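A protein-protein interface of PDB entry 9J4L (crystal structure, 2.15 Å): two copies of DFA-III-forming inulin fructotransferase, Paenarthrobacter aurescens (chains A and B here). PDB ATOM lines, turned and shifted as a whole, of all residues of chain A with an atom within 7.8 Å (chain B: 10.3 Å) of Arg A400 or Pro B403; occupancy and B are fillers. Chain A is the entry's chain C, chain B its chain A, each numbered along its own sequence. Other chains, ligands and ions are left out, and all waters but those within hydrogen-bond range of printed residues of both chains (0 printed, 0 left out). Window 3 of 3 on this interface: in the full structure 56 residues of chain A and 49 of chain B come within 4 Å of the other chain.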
ATOM      1  N   ILE A 356      23.566  -8.394 -11.228  1.00  0.00           N
ATOM      2  CA  ILE A 356      23.187  -7.036 -10.850  1.00  0.00           C
ATOM      3  C   ILE A 356      22.382  -6.507 -12.014  1.00  0.00           C
ATOM      4  O   ILE A 356      22.909  -6.362 -13.107  1.00  0.00           O
ATOM      5  CB  ILE A 356      24.411  -6.117 -10.611  1.00  0.00           C
ATOM      6  CG1 ILE A 356      25.204  -6.612  -9.401  1.00  0.00           C
ATOM      7  CG2 ILE A 356      23.970  -4.674 -10.396  1.00  0.00           C
ATOM      8  CD1 ILE A 356      26.375  -5.738  -9.001  1.00  0.00           C
ATOM      9  N   ALA A 357      21.080  -6.315 -11.813  1.00  0.00           N
ATOM     10  CA  ALA A 357      20.179  -6.069 -12.943  1.00  0.00           C
ATOM     11  C   ALA A 357      19.164  -4.972 -12.679  1.00  0.00           C
ATOM     12  O   ALA A 357      18.537  -4.924 -11.606  1.00  0.00           O
ATOM     13  CB  ALA A 357      19.490  -7.366 -13.377  1.00  0.00           C
ATOM     14  N   THR A 358      18.987  -4.113 -13.681  1.00  0.00           N
ATOM     15  CA  THR A 358      17.987  -3.035 -13.650  1.00  0.00           C
ATOM     16  C   THR A 358      17.979  -2.188 -12.349  1.00  0.00           C
ATOM     17  O   THR A 358      16.962  -2.057 -11.660  1.00  0.00           O
ATOM     18  CB  THR A 358      16.582  -3.526 -14.087  1.00  0.00           C
ATOM     19  OG1 THR A 358      15.881  -4.034 -12.961  1.00  0.00           O
ATOM     20  CG2 THR A 358      16.690  -4.663 -15.111  1.00  0.00           C
ATOM     21  N   SER A 379      30.362 -12.929 -13.000  1.00  0.00           N
ATOM     22  CA  SER A 379      29.371 -11.888 -12.723  1.00  0.00           C
ATOM     23  C   SER A 379      28.555 -11.402 -13.940  1.00  0.00           C
ATOM     24  O   SER A 379      29.053 -11.392 -15.061  1.00  0.00           O
ATOM     25  CB  SER A 379      30.061 -10.703 -12.039  1.00  0.00           C
ATOM     26  OG  SER A 379      31.008 -11.154 -11.092  1.00  0.00           O
ATOM     27  N   LYS A 380      27.310 -10.978 -13.700  1.00  0.00           N
ATOM     28  CA  LYS A 380      26.506 -10.268 -14.711  1.00  0.00           C
ATOM     29  C   LYS A 380      26.027  -8.907 -14.217  1.00  0.00           C
ATOM     30  O   LYS A 380      25.529  -8.777 -13.073  1.00  0.00           O
ATOM     31  CB  LYS A 380      25.295 -11.076 -15.187  1.00  0.00           C
ATOM     32  CG  LYS A 380      25.625 -12.259 -16.085  1.00  0.00           C
ATOM     33  CD  LYS A 380      25.890 -13.455 -15.210  1.00  0.00           C
ATOM     34  CE  LYS A 380      26.252 -14.698 -16.002  1.00  0.00           C
ATOM     35  NZ  LYS A 380      27.001 -15.598 -15.056  1.00  0.00           N
ATOM     36  N   VAL A 381      26.189  -7.907 -15.086  1.00  0.00           N
ATOM     37  CA  VAL A 381      25.697  -6.553 -14.841  1.00  0.00           C
ATOM     38  C   VAL A 381      24.822  -6.114 -16.023  1.00  0.00           C
ATOM     39  O   VAL A 381      25.336  -5.895 -17.116  1.00  0.00           O
ATOM     40  CB  VAL A 381      26.862  -5.540 -14.665  1.00  0.00           C
ATOM     41  CG1 VAL A 381      26.320  -4.156 -14.330  1.00  0.00           C
ATOM     42  CG2 VAL A 381      27.858  -5.999 -13.597  1.00  0.00           C
ATOM     43  N   LEU A 382      23.515  -5.984 -15.790  1.00  0.00           N
ATOM     44  CA  LEU A 382      22.540  -5.604 -16.813  1.00  0.00           C
ATOM     45  C   LEU A 382      21.845  -4.290 -16.441  1.00  0.00           C
ATOM     46  O   LEU A 382      21.359  -4.136 -15.304  1.00  0.00           O
ATOM     47  CB  LEU A 382      21.482  -6.709 -16.953  1.00  0.00           C
ATOM     48  CG  LEU A 382      21.990  -8.147 -17.079  1.00  0.00           C
ATOM     49  CD1 LEU A 382      20.791  -9.079 -17.221  1.00  0.00           C
ATOM     50  CD2 LEU A 382      22.914  -8.273 -18.290  1.00  0.00           C
ATOM     51  N   ASP A 383      21.858  -3.328 -17.367  1.00  0.00           N
ATOM     52  CA  ASP A 383      21.024  -2.126 -17.243  1.00  0.00           C
ATOM     53  C   ASP A 383      21.144  -1.473 -15.888  1.00  0.00           C
ATOM     54  O   ASP A 383      20.130  -1.225 -15.241  1.00  0.00           O
ATOM     55  CB  ASP A 383      19.551  -2.484 -17.451  1.00  0.00           C
ATOM     56  CG  ASP A 383      19.301  -3.164 -18.771  1.00  0.00           C
ATOM     57  OD1 ASP A 383      20.043  -2.888 -19.734  1.00  0.00           O
ATOM     58  OD2 ASP A 383      18.432  -4.041 -18.812  1.00  0.00           O
ATOM     59  N   SER A 384      22.363  -1.303 -15.394  1.00  0.00           N
ATOM     60  CA  SER A 384      22.532  -0.610 -14.134  1.00  0.00           C
ATOM     61  C   SER A 384      23.466   0.570 -14.329  1.00  0.00           C
ATOM     62  O   SER A 384      24.198   0.929 -13.415  1.00  0.00           O
ATOM     63  CB  SER A 384      23.069  -1.572 -13.054  1.00  0.00           C
ATOM     64  OG  SER A 384      22.212  -2.699 -12.906  1.00  0.00           O
ATOM     65  N   GLY A 385      23.504   1.101 -15.556  1.00  0.00           N
ATOM     66  CA  GLY A 385      24.400   2.193 -15.897  1.00  0.00           C
ATOM     67  C   GLY A 385      25.104   2.030 -17.232  1.00  0.00           C
ATOM     68  O   GLY A 385      25.162   0.931 -17.808  1.00  0.00           O
ATOM     69  N   ALA A 386      25.636   3.141 -17.740  1.00  0.00           N
ATOM     70  CA  ALA A 386      26.452   3.098 -18.943  1.00  0.00           C
ATOM     71  C   ALA A 386      27.775   2.372 -18.655  1.00  0.00           C
ATOM     72  O   ALA A 386      28.195   2.245 -17.499  1.00  0.00           O
ATOM     73  CB  ALA A 386      26.706   4.509 -19.462  1.00  0.00           C
ATOM     74  N   ALA A 387      28.421   1.901 -19.719  1.00  0.00           N
ATOM     75  CA  ALA A 387      29.722   1.254 -19.612  1.00  0.00           C
ATOM     76  C   ALA A 387      30.726   2.058 -18.770  1.00  0.00           C
ATOM     77  O   ALA A 387      31.426   1.477 -17.939  1.00  0.00           O
ATOM     78  CB  ALA A 387      30.279   0.957 -20.998  1.00  0.00           C
ATOM     79  N   ILE A 390      30.449   1.090 -14.899  1.00  0.00           N
ATOM     80  CA  ILE A 390      30.723  -0.282 -14.443  1.00  0.00           C
ATOM     81  C   ILE A 390      32.223  -0.586 -14.512  1.00  0.00           C
ATOM     82  O   ILE A 390      32.806  -0.660 -15.592  1.00  0.00           O
ATOM     83  CB  ILE A 390      29.964  -1.329 -15.304  1.00  0.00           C
ATOM     84  CG1 ILE A 390      28.518  -0.881 -15.592  1.00  0.00           C
ATOM     85  CG2 ILE A 390      30.030  -2.724 -14.671  1.00  0.00           C
ATOM     86  CD1 ILE A 390      27.679  -0.607 -14.358  1.00  0.00           C
ATOM     87  N   THR A 397      33.541 -10.507 -16.329  1.00  0.00           N
ATOM     88  CA  THR A 397      32.208  -9.978 -16.080  1.00  0.00           C
ATOM     89  C   THR A 397      31.464  -9.696 -17.399  1.00  0.00           C
ATOM     90  O   THR A 397      31.974  -8.977 -18.256  1.00  0.00           O
ATOM     91  CB  THR A 397      32.322  -8.664 -15.293  1.00  0.00           C
ATOM     92  OG1 THR A 397      33.036  -8.899 -14.073  1.00  0.00           O
ATOM     93  CG2 THR A 397      30.959  -8.097 -14.983  1.00  0.00           C
ATOM     94  N   ALA A 398      30.261 -10.244 -17.553  1.00  0.00           N
ATOM     95  CA  ALA A 398      29.393  -9.877 -18.682  1.00  0.00           C
ATOM     96  C   ALA A 398      28.631  -8.594 -18.368  1.00  0.00           C
ATOM     97  O   ALA A 398      28.051  -8.454 -17.294  1.00  0.00           O
ATOM     98  CB  ALA A 398      28.427 -11.004 -19.013  1.00  0.00           C
ATOM     99  N   ILE A 399      28.750  -7.605 -19.245  1.00  0.00           N
ATOM    100  CA  ILE A 399      28.174  -6.288 -19.002  1.00  0.00           C
ATOM    101  C   ILE A 399      27.277  -5.868 -20.164  1.00  0.00           C
ATOM    102  O   ILE A 399      27.761  -5.705 -21.281  1.00  0.00           O
ATOM    103  CB  ILE A 399      29.262  -5.212 -18.811  1.00  0.00           C
ATOM    104  CG1 ILE A 399      30.216  -5.613 -17.675  1.00  0.00           C
ATOM    105  CG2 ILE A 399      28.613  -3.854 -18.569  1.00  0.00           C
ATOM    106  CD1 ILE A 399      31.416  -4.711 -17.496  1.00  0.00           C
ATOM    107  N   ARG A 400      26.006  -5.629 -19.922  1.00  0.00           N
ATOM    108  CA  ARG A 400      25.164  -4.877 -20.814  1.00  0.00           C
ATOM    109  C   ARG A 400      24.952  -3.464 -20.301  1.00  0.00           C
ATOM    110  O   ARG A 400      24.323  -3.299 -19.315  1.00  0.00           O
ATOM    111  CB  ARG A 400      23.820  -5.565 -20.995  1.00  0.00           C
ATOM    112  CG  ARG A 400      22.997  -4.972 -22.106  1.00  0.00           C
ATOM    113  CD  ARG A 400      21.767  -5.780 -22.435  1.00  0.00           C
ATOM    114  NE  ARG A 400      20.839  -5.804 -21.351  1.00  0.00           N
ATOM    115  CZ  ARG A 400      20.066  -6.821 -21.044  1.00  0.00           C
ATOM    116  NH1 ARG A 400      20.044  -7.901 -21.764  1.00  0.00           N
ATOM    117  NH2 ARG A 400      19.267  -6.727 -20.048  1.00  0.00           N
ATOM    118  N   PRO A 401      25.463  -2.475 -20.985  1.00  0.00           N
ATOM    119  CA  PRO A 401      25.165  -1.138 -20.546  1.00  0.00           C
ATOM    120  C   PRO A 401      23.691  -0.781 -20.785  1.00  0.00           C
ATOM    121  O   PRO A 401      23.066  -1.204 -21.706  1.00  0.00           O
ATOM    122  CB  PRO A 401      26.126  -0.265 -21.349  1.00  0.00           C
ATOM    123  CG  PRO A 401      26.859  -1.156 -22.217  1.00  0.00           C
ATOM    124  CD  PRO A 401      26.193  -2.478 -22.235  1.00  0.00           C
ATOM    125  N   THR A 402      23.179  -0.013 -19.859  1.00  0.00           N
ATOM    126  CA  THR A 402      21.961   0.698 -20.013  1.00  0.00           C
ATOM    127  C   THR A 402      21.958   1.396 -21.367  1.00  0.00           C
ATOM    128  O   THR A 402      22.864   2.099 -21.702  1.00  0.00           O
ATOM    129  CB  THR A 402      21.732   1.715 -18.894  1.00  0.00           C
ATOM    130  OG1 THR A 402      21.673   1.072 -17.642  1.00  0.00           O
ATOM    131  CG2 THR A 402      20.443   2.455 -19.130  1.00  0.00           C
ATOM    132  N   PRO A 403      20.927   1.178 -22.178  1.00  0.00           N
ATOM    133  CA  PRO A 403      20.815   1.894 -23.443  1.00  0.00           C
ATOM    134  C   PRO A 403      20.774   3.389 -23.260  1.00  0.00           C
ATOM    135  O   PRO A 403      21.514   3.886 -24.049  1.00  0.00           O
ATOM    136  CB  PRO A 403      19.484   1.435 -24.012  1.00  0.00           C
ATOM    137  CG  PRO A 403      19.243   0.149 -23.406  1.00  0.00           C
ATOM    138  CD  PRO A 403      19.908   0.144 -22.067  1.00  0.00           C
ATOM    139  N   ALA B 357      10.854 -12.415 -17.016  1.00  0.00           N
ATOM    140  CA  ALA B 357      11.904 -11.394 -17.165  1.00  0.00           C
ATOM    141  C   ALA B 357      12.769 -11.232 -15.926  1.00  0.00           C
ATOM    142  O   ALA B 357      12.248 -11.125 -14.820  1.00  0.00           O
ATOM    143  CB  ALA B 357      11.287 -10.045 -17.560  1.00  0.00           C
ATOM    144  N   THR B 358      14.084 -11.171 -16.125  1.00  0.00           N
ATOM    145  CA  THR B 358      15.031 -10.840 -15.062  1.00  0.00           C
ATOM    146  C   THR B 358      14.921 -11.779 -13.859  1.00  0.00           C
ATOM    147  O   THR B 358      14.662 -11.336 -12.745  1.00  0.00           O
ATOM    148  CB  THR B 358      14.858  -9.384 -14.565  1.00  0.00           C
ATOM    149  OG1 THR B 358      14.414  -8.542 -15.644  1.00  0.00           O
ATOM    150  CG2 THR B 358      16.189  -8.847 -14.007  1.00  0.00           C
ATOM    151  N   ASN B 359      15.045 -13.077 -14.104  1.00  0.00           N
ATOM    152  CA  ASN B 359      14.998 -14.077 -13.047  1.00  0.00           C
ATOM    153  C   ASN B 359      16.375 -14.744 -12.920  1.00  0.00           C
ATOM    154  O   ASN B 359      17.002 -15.123 -13.930  1.00  0.00           O
ATOM    155  CB  ASN B 359      13.923 -15.137 -13.370  1.00  0.00           C
ATOM    156  CG  ASN B 359      12.523 -14.555 -13.403  1.00  0.00           C
ATOM    157  OD1 ASN B 359      12.004 -14.129 -12.375  1.00  0.00           O
ATOM    158  ND2 ASN B 359      11.935 -14.461 -14.588  1.00  0.00           N
ATOM    159  N   VAL B 381      10.640 -14.183 -23.071  1.00  0.00           N
ATOM    160  CA  VAL B 381      11.588 -14.631 -22.056  1.00  0.00           C
ATOM    161  C   VAL B 381      12.812 -13.726 -22.135  1.00  0.00           C
ATOM    162  O   VAL B 381      13.460 -13.593 -23.182  1.00  0.00           O
ATOM    163  CB  VAL B 381      11.991 -16.119 -22.235  1.00  0.00           C
ATOM    164  CG1 VAL B 381      12.974 -16.545 -21.143  1.00  0.00           C
ATOM    165  CG2 VAL B 381      10.754 -17.012 -22.232  1.00  0.00           C
ATOM    166  N   LEU B 382      13.023 -12.973 -21.070  1.00  0.00           N
ATOM    167  CA  LEU B 382      14.071 -11.971 -21.054  1.00  0.00           C
ATOM    168  C   LEU B 382      14.966 -12.215 -19.852  1.00  0.00           C
ATOM    169  O   LEU B 382      14.479 -12.255 -18.715  1.00  0.00           O
ATOM    170  CB  LEU B 382      13.456 -10.578 -20.936  1.00  0.00           C
ATOM    171  CG  LEU B 382      12.394 -10.152 -21.947  1.00  0.00           C
ATOM    172  CD1 LEU B 382      11.913  -8.743 -21.611  1.00  0.00           C
ATOM    173  CD2 LEU B 382      12.987 -10.218 -23.344  1.00  0.00           C
ATOM    174  N   ASP B 383      16.270 -12.335 -20.094  1.00  0.00           N
ATOM    175  CA  ASP B 383      17.250 -12.283 -19.004  1.00  0.00           C
ATOM    176  C   ASP B 383      16.897 -13.247 -17.867  1.00  0.00           C
ATOM    177  O   ASP B 383      17.042 -12.940 -16.680  1.00  0.00           O
ATOM    178  CB  ASP B 383      17.363 -10.841 -18.500  1.00  0.00           C
ATOM    179  CG  ASP B 383      17.702  -9.854 -19.627  1.00  0.00           C
ATOM    180  OD1 ASP B 383      18.361 -10.245 -20.611  1.00  0.00           O
ATOM    181  OD2 ASP B 383      17.324  -8.671 -19.533  1.00  0.00           O
ATOM    182  N   SER B 384      16.443 -14.433 -18.239  1.00  0.00           N
ATOM    183  CA  SER B 384      16.118 -15.440 -17.254  1.00  0.00           C
ATOM    184  C   SER B 384      16.919 -16.719 -17.477  1.00  0.00           C
ATOM    185  O   SER B 384      16.516 -17.813 -17.026  1.00  0.00           O
ATOM    186  CB  SER B 384      14.614 -15.719 -17.254  1.00  0.00           C
ATOM    187  OG  SER B 384      13.909 -14.523 -16.965  1.00  0.00           O
ATOM    188  N   GLY B 385      18.069 -16.563 -18.139  1.00  0.00           N
ATOM    189  CA  GLY B 385      19.009 -17.663 -18.355  1.00  0.00           C
ATOM    190  C   GLY B 385      19.736 -17.538 -19.677  1.00  0.00           C
ATOM    191  O   GLY B 385      19.294 -16.799 -20.568  1.00  0.00           O
ATOM    192  N   ALA B 386      20.855 -18.253 -19.810  1.00  0.00           N
ATOM    193  CA  ALA B 386      21.498 -18.428 -21.117  1.00  0.00           C
ATOM    194  C   ALA B 386      20.576 -19.169 -22.085  1.00  0.00           C
ATOM    195  O   ALA B 386      19.633 -19.842 -21.662  1.00  0.00           O
ATOM    196  CB  ALA B 386      22.808 -19.177 -20.965  1.00  0.00           C
ATOM    197  N   ALA B 387      20.843 -19.040 -23.383  1.00  0.00           N
ATOM    198  CA  ALA B 387      20.063 -19.742 -24.407  1.00  0.00           C
ATOM    199  C   ALA B 387      19.845 -21.233 -24.117  1.00  0.00           C
ATOM    200  O   ALA B 387      18.773 -21.779 -24.412  1.00  0.00           O
ATOM    201  CB  ALA B 387      20.708 -19.566 -25.769  1.00  0.00           C
ATOM    202  N   SER B 388      20.870 -21.892 -23.573  1.00  0.00           N
ATOM    203  CA  SER B 388      20.824 -23.329 -23.336  1.00  0.00           C
ATOM    204  C   SER B 388      19.874 -23.691 -22.187  1.00  0.00           C
ATOM    205  O   SER B 388      19.556 -24.861 -21.984  1.00  0.00           O
ATOM    206  CB  SER B 388      22.232 -23.864 -23.047  1.00  0.00           C
ATOM    207  OG  SER B 388      23.080 -22.822 -22.585  1.00  0.00           O
ATOM    208  N   THR B 389      19.478 -22.698 -21.392  1.00  0.00           N
ATOM    209  CA  THR B 389      18.575 -22.930 -20.266  1.00  0.00           C
ATOM    210  C   THR B 389      17.100 -22.604 -20.604  1.00  0.00           C
ATOM    211  O   THR B 389      16.196 -22.876 -19.807  1.00  0.00           O
ATOM    212  CB  THR B 389      19.064 -22.190 -18.994  1.00  0.00           C
ATOM    213  OG1 THR B 389      18.993 -20.769 -19.200  1.00  0.00           O
ATOM    214  CG2 THR B 389      20.523 -22.552 -18.678  1.00  0.00           C
ATOM    215  N   ILE B 390      16.869 -22.031 -21.757  1.00  0.00           N
ATOM    216  CA  ILE B 390      15.516 -21.785 -22.242  1.00  0.00           C
ATOM    217  C   ILE B 390      15.017 -22.776 -23.303  1.00  0.00           C
ATOM    218  O   ILE B 390      15.624 -22.934 -24.305  1.00  0.00           O
ATOM    219  CB  ILE B 390      15.316 -20.337 -22.726  1.00  0.00           C
ATOM    220  CG1 ILE B 390      16.052 -19.360 -21.812  1.00  0.00           C
ATOM    221  CG2 ILE B 390      13.862 -19.990 -22.883  1.00  0.00           C
ATOM    222  CD1 ILE B 390      15.510 -19.258 -20.430  1.00  0.00           C
ATOM    223  N   ILE B 399      12.954 -14.664 -27.267  1.00  0.00           N
ATOM    224  CA  ILE B 399      13.903 -14.962 -26.194  1.00  0.00           C
ATOM    225  C   ILE B 399      15.136 -14.060 -26.273  1.00  0.00           C
ATOM    226  O   ILE B 399      15.895 -14.114 -27.232  1.00  0.00           O
ATOM    227  CB  ILE B 399      14.403 -16.432 -26.275  1.00  0.00           C
ATOM    228  CG1 ILE B 399      13.251 -17.429 -26.213  1.00  0.00           C
ATOM    229  CG2 ILE B 399      15.412 -16.729 -25.176  1.00  0.00           C
ATOM    230  CD1 ILE B 399      13.641 -18.839 -26.644  1.00  0.00           C
ATOM    231  N   ARG B 400      15.392 -13.292 -25.223  1.00  0.00           N
ATOM    232  CA  ARG B 400      16.701 -12.697 -25.032  1.00  0.00           C
ATOM    233  C   ARG B 400      17.492 -13.459 -23.954  1.00  0.00           C
ATOM    234  O   ARG B 400      17.074 -13.497 -22.777  1.00  0.00           O
ATOM    235  CB  ARG B 400      16.580 -11.200 -24.695  1.00  0.00           C
ATOM    236  CG  ARG B 400      17.925 -10.512 -24.468  1.00  0.00           C
ATOM    237  CD  ARG B 400      17.756  -9.023 -24.231  1.00  0.00           C
ATOM    238  NE  ARG B 400      16.476  -8.756 -23.589  1.00  0.00           N
ATOM    239  CZ  ARG B 400      16.240  -7.736 -22.782  1.00  0.00           C
ATOM    240  NH1 ARG B 400      17.202  -6.882 -22.497  1.00  0.00           N
ATOM    241  NH2 ARG B 400      15.056  -7.589 -22.230  1.00  0.00           N
ATOM    242  N   PRO B 401      18.599 -14.127 -24.360  1.00  0.00           N
ATOM    243  CA  PRO B 401      19.466 -14.790 -23.368  1.00  0.00           C
ATOM    244  C   PRO B 401      20.051 -13.779 -22.388  1.00  0.00           C
ATOM    245  O   PRO B 401      20.268 -12.623 -22.739  1.00  0.00           O
ATOM    246  CB  PRO B 401      20.600 -15.411 -24.214  1.00  0.00           C
ATOM    247  CG  PRO B 401      20.174 -15.289 -25.644  1.00  0.00           C
ATOM    248  CD  PRO B 401      19.170 -14.173 -25.724  1.00  0.00           C
ATOM    249  N   THR B 402      20.281 -14.203 -21.156  1.00  0.00           N
ATOM    250  CA  THR B 402      21.172 -13.481 -20.279  1.00  0.00           C
ATOM    251  C   THR B 402      22.529 -13.385 -20.994  1.00  0.00           C
ATOM    252  O   THR B 402      23.043 -14.383 -21.493  1.00  0.00           O
ATOM    253  CB  THR B 402      21.286 -14.200 -18.917  1.00  0.00           C
ATOM    254  OG1 THR B 402      19.970 -14.412 -18.374  1.00  0.00           O
ATOM    255  CG2 THR B 402      22.102 -13.381 -17.936  1.00  0.00           C
ATOM    256  N   PRO B 403      23.065 -12.161 -21.143  1.00  0.00           N
ATOM    257  CA  PRO B 403      24.341 -11.948 -21.843  1.00  0.00           C
ATOM    258  C   PRO B 403      25.483 -12.829 -21.320  1.00  0.00           C
ATOM    259  O   PRO B 403      25.544 -13.091 -20.117  1.00  0.00           O
ATOM    260  CB  PRO B 403      24.658 -10.479 -21.550  1.00  0.00           C
ATOM    261  CG  PRO B 403      23.338  -9.847 -21.301  1.00  0.00           C
ATOM    262  CD  PRO B 403      22.486 -10.900 -20.647  1.00  0.00           C
ATOM    263  N   HIS B 404      26.463 -13.066 -22.197  1.00  0.00           N
ATOM    264  CA  HIS B 404      27.564 -14.040 -22.046  1.00  0.00           C
ATOM    265  C   HIS B 404      27.279 -15.419 -21.538  1.00  0.00           C
ATOM    266  O   HIS B 404      27.373 -16.381 -22.294  1.00  0.00           O
ATOM    267  CB  HIS B 404      28.808 -13.445 -21.394  1.00  0.00           C
ATOM    268  CG  HIS B 404      30.018 -13.444 -22.300  1.00  0.00           C
ATOM    269  ND1 HIS B 404      30.589 -14.585 -22.745  1.00  0.00           N
ATOM    270  CD2 HIS B 404      30.690 -12.395 -22.931  1.00  0.00           C
ATOM    271  CE1 HIS B 404      31.578 -14.284 -23.610  1.00  0.00           C
ATOM    272  NE2 HIS B 404      31.641 -12.942 -23.722  1.00  0.00           N
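Of the 20 printed residues of chain A, 4 touch a printed residue of chain B.
Hydrophobic or aromatic side chains of chain A that line the printed part of chain B: Ala A357, Leu A382 and Ala A398.
Along chain A the printed residues that touch a printed residue of chain B span positions 357 to 400.
Of the 19 printed residues of chain B, 5 touch a printed residue of chain A.
Hydrophobic or aromatic side chains of chain B within 4 Å of the printed part of chain A: Pro B403 and His B404.
Among the printed residues, 8 pairs touch across the chains.
Among the printed residues, Asp or Glu carboxylates within 4 Å of a Lys or Arg side-chain nitrogen of the other chain: Arg A400 with Asp B383 (2.8 Å).
Among the printed residues, pairs that only touch across the chains: Leu A382 with Pro B403 (3.4 Å), Ala A398 with His B404 (3.4 Å), Ala A357 with Thr B358 (3.7 Å), Ala A398 with Pro B403 (3.7 Å), Arg A400 with Pro B403 (3.9 Å) and Leu A382 with Asp B383 (3.99 Å).
Leu A382 touches Asp B383, but with the chains exchanged Asp A383 does not touch Leu B382 (8.5 Å).
Leu A382 touches Pro B403, but with the chains exchanged Pro A403 does not touch Leu B382 (11.7 Å).
Arg A400 touches Asp B383, but with the chains exchanged Asp A383 does not touch Arg B400 (4.8 Å).
Arg B400 touches its own counterpart, Arg A400.
Of the 8 pairs that touch across the chains among the printed residues, 1 has its exchanged pair printed and touching as well.
The backbone carbonyl oxygen (O) of Leu A382 is in hydrogen-bond range of the backbone NH (N) of Thr A358 (2.9 Å).
The backbone carbonyl oxygen (O) of Val A381 sits at hydrogen-bond distance from the backbone NH (N) of Arg A400.
The backbone NH of Asn B359 lies within hydrogen-bond range of the backbone carbonyl oxygen of Asp B383 (3.3 Å).
The side-chain hydroxyl (OG) of Ser A384 sits at hydrogen-bond distance from the backbone carbonyl oxygen (O) of Leu A382 (2.9 Å).
OG of Ser B384 lies within hydrogen-bond range of N of Thr B358 (3.5 Å).
N of Arg B400 lies within hydrogen-bond range of O of Val B381 (2.8 Å).
The guanidinium group (NH1) of Arg A400 sits close to the guanidinium group (NH1) of Arg B400.
The side-chain carboxylate of Asp B383 lies within salt-bridge range of the guanidinium group of Arg A400, at 2.8 Å.
Of the printed residues of chain B, Leu A382 touches Asp B383 (3.99 Å) and Pro B403 (3.4 Å).
No residue of chain B comes within 4 Å of Asp A383.
Arg A400 touches just these residues of chain B: Asp B383 (2.8 Å), Arg B400 (3.1 Å) and Pro B403 (3.9 Å).
No residue of chain B comes within 4 Å of Pro A401.
Pro A403 touches none of the printed residues of chain B.
Of the printed residues of chain A, Thr B358 touches Ala A357.
Printed residues of chain A within 4 Å of Asp B383: Leu A382 and Arg A400.
Pro B403 touches just these residues of chain A: Leu A382, Ala A398 and Arg A400.
The nearest residue of chain B that does not touch Arg A400 is Pro B401 (4.8 Å).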
